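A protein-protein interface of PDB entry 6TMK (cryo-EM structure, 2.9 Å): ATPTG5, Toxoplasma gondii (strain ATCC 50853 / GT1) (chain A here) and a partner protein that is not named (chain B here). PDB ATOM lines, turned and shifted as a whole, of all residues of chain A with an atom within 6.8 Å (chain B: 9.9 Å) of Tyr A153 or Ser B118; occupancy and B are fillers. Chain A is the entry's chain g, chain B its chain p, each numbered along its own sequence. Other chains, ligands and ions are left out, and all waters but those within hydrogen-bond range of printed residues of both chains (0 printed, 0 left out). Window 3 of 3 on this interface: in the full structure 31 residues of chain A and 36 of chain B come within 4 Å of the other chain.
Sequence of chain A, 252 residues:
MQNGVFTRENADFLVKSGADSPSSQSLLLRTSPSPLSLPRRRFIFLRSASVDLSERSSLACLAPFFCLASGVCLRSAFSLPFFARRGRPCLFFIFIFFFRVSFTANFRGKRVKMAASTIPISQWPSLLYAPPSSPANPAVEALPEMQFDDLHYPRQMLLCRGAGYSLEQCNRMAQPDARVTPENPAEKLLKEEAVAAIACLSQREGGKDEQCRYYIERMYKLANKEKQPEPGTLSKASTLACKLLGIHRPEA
NH2 of Arg B74 is in hydrogen-bond range of O of Pro A176, at 2.4 Å. OD1 of Asn A171 sits close to O of Phe B120, at 3.2 Å.
OE2 of Glu B71 lies within salt-bridge range of NH1 of Arg B75 (3.7 Å). The side-chain amide oxygen (OE1) of Gln A156 lies close to the backbone carbonyl oxygen (O) of Gln A175, 3.4 Å away. N of Phe B120 sits close to OG of Ser B118 (3.4 Å). A ring nitrogen (NE2) of His A152 lies within hydrogen-bond range of the backbone carbonyl oxygen (O) of Gln A175, at 2.7 Å. The backbone NH of Asp A177 is in hydrogen-bond range of a ring nitrogen (NE2) of His A152 (3.2 Å).
Among the printed residues, pairs that only touch across the chains: Tyr A153 with Leu B117 (3.8 Å), Tyr A153 with Ser B118 (3.5 Å), Asn A171 with Ala B121 (3.9 Å), Gln A175 with Arg B74 (3.8 Å), Pro A176 with Arg B75 (3.9 Å) and Asp A177 with Phe B78 (3.7 Å).
Tyr A153 touches just these residues of chain B: Leu B117 and Ser B118. Printed residues of chain A within 4 Å of Ser B118: Tyr A153 (3.5 Å). No residue of chain B comes within 4 Å of His A152. Of chain B, only Arg B74 and Arg B75 come within 4 Å of Pro A176. Printed residues of chain B within 4 Å of Asn A171: Phe B120 and Ala B121. Printed residues of chain A within 4 Å of Arg B75: Pro A176 (3.9 Å). Printed residues of chain A within 4 Å of Leu B117: Tyr A153. Printed residues of chain B within 4 Å of Asp A177: Phe B78. Printed residues of chain A within 4 Å of Phe B78: Asp A177 (3.7 Å). Leu A158 touches none of the printed residues of chain B. The nearest residue of chain A that does not touch Ser B118 is Asn A171 (4.4 Å). The nearest printed residue of chain A that does not touch Leu B117 is Pro A176 (4.4 Å).
Printed residues of chain A that touch a printed residue of chain B: Tyr A153, Asn A171, Gln A175, Pro A176 and Asp A177. Hydrophobic or aromatic side chains of chain A that line the printed part of chain B: Tyr A153 and Pro A176. Along chain A the printed residues that touch a printed residue of chain B span positions 153 to 177. Hydrophobic or aromatic side chains of chain B that line the printed part of chain A: Phe B78, Leu B117 and Phe B120. Among the printed residues, no Asp or Glu carboxylate lies within 4 Å of a Lys or Arg side-chain nitrogen of the other chain.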
ATOM      1  N   ASP A 149      12.108   2.584 -19.314  1.00  0.00           N
ATOM      2  CA  ASP A 149      13.492   3.003 -19.147  1.00  0.00           C
ATOM      3  C   ASP A 149      13.721   3.496 -17.725  1.00  0.00           C
ATOM      4  O   ASP A 149      13.069   4.445 -17.276  1.00  0.00           O
ATOM      5  CB  ASP A 149      13.847   4.097 -20.153  1.00  0.00           C
ATOM      6  CG  ASP A 149      15.279   4.009 -20.633  1.00  0.00           C
ATOM      7  OD1 ASP A 149      16.083   3.301 -19.996  1.00  0.00           O
ATOM      8  OD2 ASP A 149      15.600   4.656 -21.651  1.00  0.00           O
ATOM      9  N   ASP A 150      14.647   2.849 -17.023  1.00  0.00           N
ATOM     10  CA  ASP A 150      15.100   3.323 -15.728  1.00  0.00           C
ATOM     11  C   ASP A 150      16.138   4.431 -15.842  1.00  0.00           C
ATOM     12  O   ASP A 150      16.483   5.041 -14.824  1.00  0.00           O
ATOM     13  CB  ASP A 150      15.684   2.161 -14.929  1.00  0.00           C
ATOM     14  CG  ASP A 150      14.639   1.140 -14.531  1.00  0.00           C
ATOM     15  OD1 ASP A 150      13.697   1.500 -13.794  1.00  0.00           O
ATOM     16  OD2 ASP A 150      14.762  -0.028 -14.951  1.00  0.00           O
ATOM     17  N   LEU A 151      16.643   4.698 -17.044  1.00  0.00           N
ATOM     18  CA  LEU A 151      17.660   5.710 -17.274  1.00  0.00           C
ATOM     19  C   LEU A 151      17.094   7.005 -17.833  1.00  0.00           C
ATOM     20  O   LEU A 151      17.859   7.921 -18.143  1.00  0.00           O
ATOM     21  CB  LEU A 151      18.713   5.171 -18.234  1.00  0.00           C
ATOM     22  CG  LEU A 151      19.730   4.179 -17.696  1.00  0.00           C
ATOM     23  CD1 LEU A 151      20.532   3.626 -18.841  1.00  0.00           C
ATOM     24  CD2 LEU A 151      20.635   4.846 -16.706  1.00  0.00           C
ATOM     25  N   HIS A 152      15.773   7.110 -17.947  1.00  0.00           N
ATOM     26  CA  HIS A 152      15.166   8.235 -18.645  1.00  0.00           C
ATOM     27  C   HIS A 152      15.481   9.552 -17.951  1.00  0.00           C
ATOM     28  O   HIS A 152      16.059  10.467 -18.550  1.00  0.00           O
ATOM     29  CB  HIS A 152      13.659   8.011 -18.744  1.00  0.00           C
ATOM     30  CG  HIS A 152      12.900   9.210 -19.210  1.00  0.00           C
ATOM     31  ND1 HIS A 152      13.140   9.816 -20.423  1.00  0.00           N
ATOM     32  CD2 HIS A 152      11.897   9.907 -18.632  1.00  0.00           C
ATOM     33  CE1 HIS A 152      12.322  10.842 -20.566  1.00  0.00           C
ATOM     34  NE2 HIS A 152      11.558  10.920 -19.493  1.00  0.00           N
ATOM     35  N   TYR A 153      15.131   9.655 -16.681  1.00  0.00           N
ATOM     36  CA  TYR A 153      15.286  10.886 -15.925  1.00  0.00           C
ATOM     37  C   TYR A 153      16.748  11.169 -15.602  1.00  0.00           C
ATOM     38  O   TYR A 153      17.183  12.324 -15.690  1.00  0.00           O
ATOM     39  CB  TYR A 153      14.459  10.817 -14.645  1.00  0.00           C
ATOM     40  CG  TYR A 153      12.991  11.086 -14.854  1.00  0.00           C
ATOM     41  CD1 TYR A 153      12.541  12.350 -15.186  1.00  0.00           C
ATOM     42  CD2 TYR A 153      12.057  10.077 -14.720  1.00  0.00           C
ATOM     43  CE1 TYR A 153      11.208  12.599 -15.377  1.00  0.00           C
ATOM     44  CE2 TYR A 153      10.722  10.320 -14.911  1.00  0.00           C
ATOM     45  CZ  TYR A 153      10.303  11.583 -15.237  1.00  0.00           C
ATOM     46  OH  TYR A 153       8.968  11.829 -15.428  1.00  0.00           O
ATOM     47  N   PRO A 154      17.535  10.165 -15.220  1.00  0.00           N
ATOM     48  CA  PRO A 154      18.978  10.412 -15.072  1.00  0.00           C
ATOM     49  C   PRO A 154      19.630  10.941 -16.336  1.00  0.00           C
ATOM     50  O   PRO A 154      20.412  11.897 -16.278  1.00  0.00           O
ATOM     51  CB  PRO A 154      19.515   9.033 -14.686  1.00  0.00           C
ATOM     52  CG  PRO A 154      18.402   8.359 -14.033  1.00  0.00           C
ATOM     53  CD  PRO A 154      17.144   8.867 -14.649  1.00  0.00           C
ATOM     54  N   ARG A 155      19.337  10.329 -17.482  1.00  0.00           N
ATOM     55  CA  ARG A 155      19.886  10.796 -18.749  1.00  0.00           C
ATOM     56  C   ARG A 155      19.439  12.217 -19.059  1.00  0.00           C
ATOM     57  O   ARG A 155      20.240  13.053 -19.493  1.00  0.00           O
ATOM     58  CB  ARG A 155      19.453   9.846 -19.855  1.00  0.00           C
ATOM     59  CG  ARG A 155      19.837  10.264 -21.243  1.00  0.00           C
ATOM     60  CD  ARG A 155      19.743   9.085 -22.159  1.00  0.00           C
ATOM     61  NE  ARG A 155      18.507   8.344 -21.935  1.00  0.00           N
ATOM     62  CZ  ARG A 155      18.401   7.021 -21.935  1.00  0.00           C
ATOM     63  NH1 ARG A 155      19.454   6.254 -22.153  1.00  0.00           N
ATOM     64  NH2 ARG A 155      17.223   6.464 -21.718  1.00  0.00           N
ATOM     65  N   GLN A 156      18.149  12.499 -18.869  1.00  0.00           N
ATOM     66  CA  GLN A 156      17.629  13.841 -19.099  1.00  0.00           C
ATOM     67  C   GLN A 156      18.362  14.869 -18.247  1.00  0.00           C
ATOM     68  O   GLN A 156      18.790  15.920 -18.744  1.00  0.00           O
ATOM     69  CB  GLN A 156      16.131  13.841 -18.804  1.00  0.00           C
ATOM     70  CG  GLN A 156      15.353  14.991 -19.382  1.00  0.00           C
ATOM     71  CD  GLN A 156      13.868  14.713 -19.370  1.00  0.00           C
ATOM     72  OE1 GLN A 156      13.391  13.885 -18.598  1.00  0.00           O
ATOM     73  NE2 GLN A 156      13.129  15.393 -20.235  1.00  0.00           N
ATOM     74  N   MET A 157      18.522  14.575 -16.956  1.00  0.00           N
ATOM     75  CA  MET A 157      19.208  15.496 -16.060  1.00  0.00           C
ATOM     76  C   MET A 157      20.653  15.689 -16.478  1.00  0.00           C
ATOM     77  O   MET A 157      21.164  16.812 -16.467  1.00  0.00           O
ATOM     78  CB  MET A 157      19.130  14.991 -14.623  1.00  0.00           C
ATOM     79  CG  MET A 157      19.807  15.894 -13.612  1.00  0.00           C
ATOM     80  SD  MET A 157      19.166  17.572 -13.585  1.00  0.00           S
ATOM     81  CE  MET A 157      17.500  17.258 -13.045  1.00  0.00           C
ATOM     82  N   LEU A 158      21.332  14.603 -16.830  1.00  0.00           N
ATOM     83  CA  LEU A 158      22.728  14.700 -17.224  1.00  0.00           C
ATOM     84  C   LEU A 158      22.877  15.574 -18.458  1.00  0.00           C
ATOM     85  O   LEU A 158      23.738  16.458 -18.510  1.00  0.00           O
ATOM     86  CB  LEU A 158      23.285  13.306 -17.484  1.00  0.00           C
ATOM     87  CG  LEU A 158      24.754  13.228 -17.861  1.00  0.00           C
ATOM     88  CD1 LEU A 158      25.603  13.637 -16.693  1.00  0.00           C
ATOM     89  CD2 LEU A 158      25.085  11.836 -18.284  1.00  0.00           C
ATOM     90  N   ASN A 171      14.297  20.344 -13.640  1.00  0.00           N
ATOM     91  CA  ASN A 171      13.076  19.745 -13.116  1.00  0.00           C
ATOM     92  C   ASN A 171      11.833  20.356 -13.745  1.00  0.00           C
ATOM     93  O   ASN A 171      10.815  19.670 -13.892  1.00  0.00           O
ATOM     94  CB  ASN A 171      13.024  19.894 -11.599  1.00  0.00           C
ATOM     95  CG  ASN A 171      13.891  18.884 -10.887  1.00  0.00           C
ATOM     96  OD1 ASN A 171      14.162  17.802 -11.404  1.00  0.00           O
ATOM     97  ND2 ASN A 171      14.327  19.229  -9.686  1.00  0.00           N
ATOM     98  N   ALA A 174      11.709  18.779 -17.288  1.00  0.00           N
ATOM     99  CA  ALA A 174      11.604  17.330 -17.336  1.00  0.00           C
ATOM    100  C   ALA A 174      10.209  16.895 -17.759  1.00  0.00           C
ATOM    101  O   ALA A 174       9.206  17.508 -17.387  1.00  0.00           O
ATOM    102  CB  ALA A 174      11.943  16.724 -15.979  1.00  0.00           C
ATOM    103  N   GLN A 175      10.157  15.818 -18.534  1.00  0.00           N
ATOM    104  CA  GLN A 175       8.922  15.229 -19.014  1.00  0.00           C
ATOM    105  C   GLN A 175       9.032  13.716 -18.917  1.00  0.00           C
ATOM    106  O   GLN A 175      10.137  13.166 -18.989  1.00  0.00           O
ATOM    107  CB  GLN A 175       8.628  15.639 -20.463  1.00  0.00           C
ATOM    108  CG  GLN A 175       8.400  17.124 -20.642  1.00  0.00           C
ATOM    109  CD  GLN A 175       8.448  17.549 -22.091  1.00  0.00           C
ATOM    110  OE1 GLN A 175       9.453  17.354 -22.774  1.00  0.00           O
ATOM    111  NE2 GLN A 175       7.357  18.129 -22.574  1.00  0.00           N
ATOM    112  N   PRO A 176       7.914  13.022 -18.751  1.00  0.00           N
ATOM    113  CA  PRO A 176       7.960  11.565 -18.625  1.00  0.00           C
ATOM    114  C   PRO A 176       8.166  10.878 -19.966  1.00  0.00           C
ATOM    115  O   PRO A 176       7.886  11.424 -21.034  1.00  0.00           O
ATOM    116  CB  PRO A 176       6.589  11.229 -18.038  1.00  0.00           C
ATOM    117  CG  PRO A 176       5.711  12.276 -18.580  1.00  0.00           C
ATOM    118  CD  PRO A 176       6.535  13.527 -18.673  1.00  0.00           C
ATOM    119  N   ASP A 177       8.668   9.651 -19.886  1.00  0.00           N
ATOM    120  CA  ASP A 177       9.104   8.943 -21.080  1.00  0.00           C
ATOM    121  C   ASP A 177       7.923   8.600 -21.972  1.00  0.00           C
ATOM    122  O   ASP A 177       6.901   8.089 -21.505  1.00  0.00           O
ATOM    123  CB  ASP A 177       9.850   7.668 -20.693  1.00  0.00           C
ATOM    124  CG  ASP A 177      10.755   7.166 -21.795  1.00  0.00           C
ATOM    125  OD1 ASP A 177      10.848   7.836 -22.844  1.00  0.00           O
ATOM    126  OD2 ASP A 177      11.373   6.097 -21.613  1.00  0.00           O
ATOM    127  N   GLU B  71       0.610  15.788 -21.900  1.00  0.00           N
ATOM    128  CA  GLU B  71       1.423  15.564 -20.711  1.00  0.00           C
ATOM    129  C   GLU B  71       0.698  14.680 -19.704  1.00  0.00           C
ATOM    130  O   GLU B  71       1.291  13.762 -19.126  1.00  0.00           O
ATOM    131  CB  GLU B  71       1.797  16.907 -20.090  1.00  0.00           C
ATOM    132  CG  GLU B  71       2.819  16.823 -18.978  1.00  0.00           C
ATOM    133  CD  GLU B  71       3.105  18.175 -18.352  1.00  0.00           C
ATOM    134  OE1 GLU B  71       2.493  19.174 -18.785  1.00  0.00           O
ATOM    135  OE2 GLU B  71       3.945  18.240 -17.429  1.00  0.00           O
ATOM    136  N   ARG B  74       0.693  11.166 -20.894  1.00  0.00           N
ATOM    137  CA  ARG B  74       2.009  10.546 -20.807  1.00  0.00           C
ATOM    138  C   ARG B  74       2.341  10.172 -19.370  1.00  0.00           C
ATOM    139  O   ARG B  74       2.907   9.105 -19.115  1.00  0.00           O
ATOM    140  CB  ARG B  74       3.068  11.476 -21.391  1.00  0.00           C
ATOM    141  CG  ARG B  74       3.302  11.261 -22.871  1.00  0.00           C
ATOM    142  CD  ARG B  74       4.138  12.361 -23.481  1.00  0.00           C
ATOM    143  NE  ARG B  74       5.493  12.371 -22.945  1.00  0.00           N
ATOM    144  CZ  ARG B  74       6.527  12.963 -23.534  1.00  0.00           C
ATOM    145  NH1 ARG B  74       6.369  13.599 -24.686  1.00  0.00           N
ATOM    146  NH2 ARG B  74       7.723  12.915 -22.971  1.00  0.00           N
ATOM    147  N   ARG B  75       1.981  11.031 -18.418  1.00  0.00           N
ATOM    148  CA  ARG B  75       2.147  10.698 -17.008  1.00  0.00           C
ATOM    149  C   ARG B  75       1.387   9.428 -16.654  1.00  0.00           C
ATOM    150  O   ARG B  75       1.932   8.512 -16.022  1.00  0.00           O
ATOM    151  CB  ARG B  75       1.660  11.852 -16.138  1.00  0.00           C
ATOM    152  CG  ARG B  75       2.526  13.080 -16.161  1.00  0.00           C
ATOM    153  CD  ARG B  75       2.398  13.849 -14.866  1.00  0.00           C
ATOM    154  NE  ARG B  75       1.036  14.308 -14.621  1.00  0.00           N
ATOM    155  CZ  ARG B  75       0.520  15.421 -15.129  1.00  0.00           C
ATOM    156  NH1 ARG B  75       1.244  16.192 -15.921  1.00  0.00           N
ATOM    157  NH2 ARG B  75      -0.726  15.763 -14.850  1.00  0.00           N
ATOM    158  N   VAL B  76       0.114   9.366 -17.038  1.00  0.00           N
ATOM    159  CA  VAL B  76      -0.703   8.218 -16.669  1.00  0.00           C
ATOM    160  C   VAL B  76      -0.204   6.956 -17.357  1.00  0.00           C
ATOM    161  O   VAL B  76      -0.210   5.869 -16.767  1.00  0.00           O
ATOM    162  CB  VAL B  76      -2.177   8.502 -16.998  1.00  0.00           C
ATOM    163  CG1 VAL B  76      -3.015   7.270 -16.776  1.00  0.00           C
ATOM    164  CG2 VAL B  76      -2.671   9.645 -16.158  1.00  0.00           C
ATOM    165  N   PHE B  78       2.933   6.364 -18.194  1.00  0.00           N
ATOM    166  CA  PHE B  78       4.146   5.989 -17.480  1.00  0.00           C
ATOM    167  C   PHE B  78       3.815   5.232 -16.202  1.00  0.00           C
ATOM    168  O   PHE B  78       4.409   4.188 -15.908  1.00  0.00           O
ATOM    169  CB  PHE B  78       4.952   7.247 -17.174  1.00  0.00           C
ATOM    170  CG  PHE B  78       6.377   6.988 -16.803  1.00  0.00           C
ATOM    171  CD1 PHE B  78       7.316   6.721 -17.773  1.00  0.00           C
ATOM    172  CD2 PHE B  78       6.779   7.028 -15.484  1.00  0.00           C
ATOM    173  CE1 PHE B  78       8.627   6.491 -17.435  1.00  0.00           C
ATOM    174  CE2 PHE B  78       8.086   6.796 -15.144  1.00  0.00           C
ATOM    175  CZ  PHE B  78       9.012   6.529 -16.119  1.00  0.00           C
ATOM    176  N   ALA B  79       2.844   5.731 -15.440  1.00  0.00           N
ATOM    177  CA  ALA B  79       2.478   5.064 -14.195  1.00  0.00           C
ATOM    178  C   ALA B  79       1.865   3.696 -14.462  1.00  0.00           C
ATOM    179  O   ALA B  79       2.138   2.726 -13.739  1.00  0.00           O
ATOM    180  CB  ALA B  79       1.521   5.940 -13.401  1.00  0.00           C
ATOM    181  N   PRO B 114      -1.515  15.940  -9.099  1.00  0.00           N
ATOM    182  CA  PRO B 114      -0.669  15.388 -10.160  1.00  0.00           C
ATOM    183  C   PRO B 114       0.489  14.571  -9.614  1.00  0.00           C
ATOM    184  O   PRO B 114       0.912  14.720  -8.466  1.00  0.00           O
ATOM    185  CB  PRO B 114      -0.171  16.634 -10.900  1.00  0.00           C
ATOM    186  CG  PRO B 114      -1.171  17.669 -10.600  1.00  0.00           C
ATOM    187  CD  PRO B 114      -1.610  17.403  -9.199  1.00  0.00           C
ATOM    188  N   PHE B 115       1.004  13.693 -10.468  1.00  0.00           N
ATOM    189  CA  PHE B 115       2.119  12.838 -10.102  1.00  0.00           C
ATOM    190  C   PHE B 115       3.447  13.556 -10.278  1.00  0.00           C
ATOM    191  O   PHE B 115       3.611  14.414 -11.148  1.00  0.00           O
ATOM    192  CB  PHE B 115       2.142  11.563 -10.939  1.00  0.00           C
ATOM    193  CG  PHE B 115       0.941  10.691 -10.770  1.00  0.00           C
ATOM    194  CD1 PHE B 115       0.247  10.659  -9.581  1.00  0.00           C
ATOM    195  CD2 PHE B 115       0.522   9.881 -11.800  1.00  0.00           C
ATOM    196  CE1 PHE B 115      -0.847   9.848  -9.434  1.00  0.00           C
ATOM    197  CE2 PHE B 115      -0.570   9.071 -11.654  1.00  0.00           C
ATOM    198  CZ  PHE B 115      -1.254   9.053 -10.470  1.00  0.00           C
ATOM    199  N   VAL B 116       4.400  13.183  -9.435  1.00  0.00           N
ATOM    200  CA  VAL B 116       5.762  13.686  -9.491  1.00  0.00           C
ATOM    201  C   VAL B 116       6.653  12.458  -9.590  1.00  0.00           C
ATOM    202  O   VAL B 116       6.989  11.838  -8.574  1.00  0.00           O
ATOM    203  CB  VAL B 116       6.118  14.541  -8.274  1.00  0.00           C
ATOM    204  CG1 VAL B 116       7.573  14.944  -8.333  1.00  0.00           C
ATOM    205  CG2 VAL B 116       5.220  15.753  -8.206  1.00  0.00           C
ATOM    206  N   LEU B 117       7.040  12.102 -10.808  1.00  0.00           N
ATOM    207  CA  LEU B 117       7.662  10.817 -11.069  1.00  0.00           C
ATOM    208  C   LEU B 117       9.180  10.871 -11.035  1.00  0.00           C
ATOM    209  O   LEU B 117       9.820   9.817 -10.974  1.00  0.00           O
ATOM    210  CB  LEU B 117       7.204  10.295 -12.429  1.00  0.00           C
ATOM    211  CG  LEU B 117       5.695  10.121 -12.566  1.00  0.00           C
ATOM    212  CD1 LEU B 117       5.282  10.241 -14.007  1.00  0.00           C
ATOM    213  CD2 LEU B 117       5.248   8.804 -11.997  1.00  0.00           C
ATOM    214  N   SER B 118       9.760  12.051 -11.082  1.00  0.00           N
ATOM    215  CA  SER B 118      11.206  12.168 -11.109  1.00  0.00           C
ATOM    216  C   SER B 118      11.781  11.950  -9.711  1.00  0.00           C
ATOM    217  O   SER B 118      11.177  12.364  -8.719  1.00  0.00           O
ATOM    218  CB  SER B 118      11.620  13.538 -11.622  1.00  0.00           C
ATOM    219  OG  SER B 118      13.006  13.587 -11.898  1.00  0.00           O
ATOM    220  N   PRO B 119      12.942  11.299  -9.602  1.00  0.00           N
ATOM    221  CA  PRO B 119      13.632  11.279  -8.306  1.00  0.00           C
ATOM    222  C   PRO B 119      14.143  12.645  -7.896  1.00  0.00           C
ATOM    223  O   PRO B 119      14.220  12.933  -6.695  1.00  0.00           O
ATOM    224  CB  PRO B 119      14.777  10.285  -8.525  1.00  0.00           C
ATOM    225  CG  PRO B 119      14.456   9.568  -9.777  1.00  0.00           C
ATOM    226  CD  PRO B 119      13.625  10.465 -10.599  1.00  0.00           C
ATOM    227  N   PHE B 120      14.496  13.490  -8.856  1.00  0.00           N
ATOM    228  CA  PHE B 120      14.937  14.846  -8.572  1.00  0.00           C
ATOM    229  C   PHE B 120      13.711  15.723  -8.360  1.00  0.00           C
ATOM    230  O   PHE B 120      12.849  15.814  -9.240  1.00  0.00           O
ATOM    231  CB  PHE B 120      15.778  15.372  -9.729  1.00  0.00           C
ATOM    232  CG  PHE B 120      16.870  14.438 -10.159  1.00  0.00           C
ATOM    233  CD1 PHE B 120      18.140  14.546  -9.632  1.00  0.00           C
ATOM    234  CD2 PHE B 120      16.625  13.454 -11.095  1.00  0.00           C
ATOM    235  CE1 PHE B 120      19.140  13.694 -10.031  1.00  0.00           C
ATOM    236  CE2 PHE B 120      17.622  12.597 -11.496  1.00  0.00           C
ATOM    237  CZ  PHE B 120      18.880  12.714 -10.959  1.00  0.00           C
ATOM    238  N   ALA B 121      13.620  16.355  -7.196  1.00  0.00           N
ATOM    239  CA  ALA B 121      12.420  17.104  -6.858  1.00  0.00           C
ATOM    240  C   ALA B 121      12.666  17.899  -5.585  1.00  0.00           C
ATOM    241  O   ALA B 121      13.493  17.515  -4.752  1.00  0.00           O
ATOM    242  CB  ALA B 121      11.225  16.166  -6.682  1.00  0.00           C
ATOM    243  N   ALA B 122      11.946  19.007  -5.451  1.00  0.00           N
ATOM    244  CA  ALA B 122      12.015  19.822  -4.245  1.00  0.00           C
ATOM    245  C   ALA B 122      10.884  20.845  -4.213  1.00  0.00           C
ATOM    246  O   ALA B 122      10.758  21.613  -3.260  1.00  0.00           O
ATOM    247  CB  ALA B 122      13.359  20.519  -4.155  1.00  0.00           C
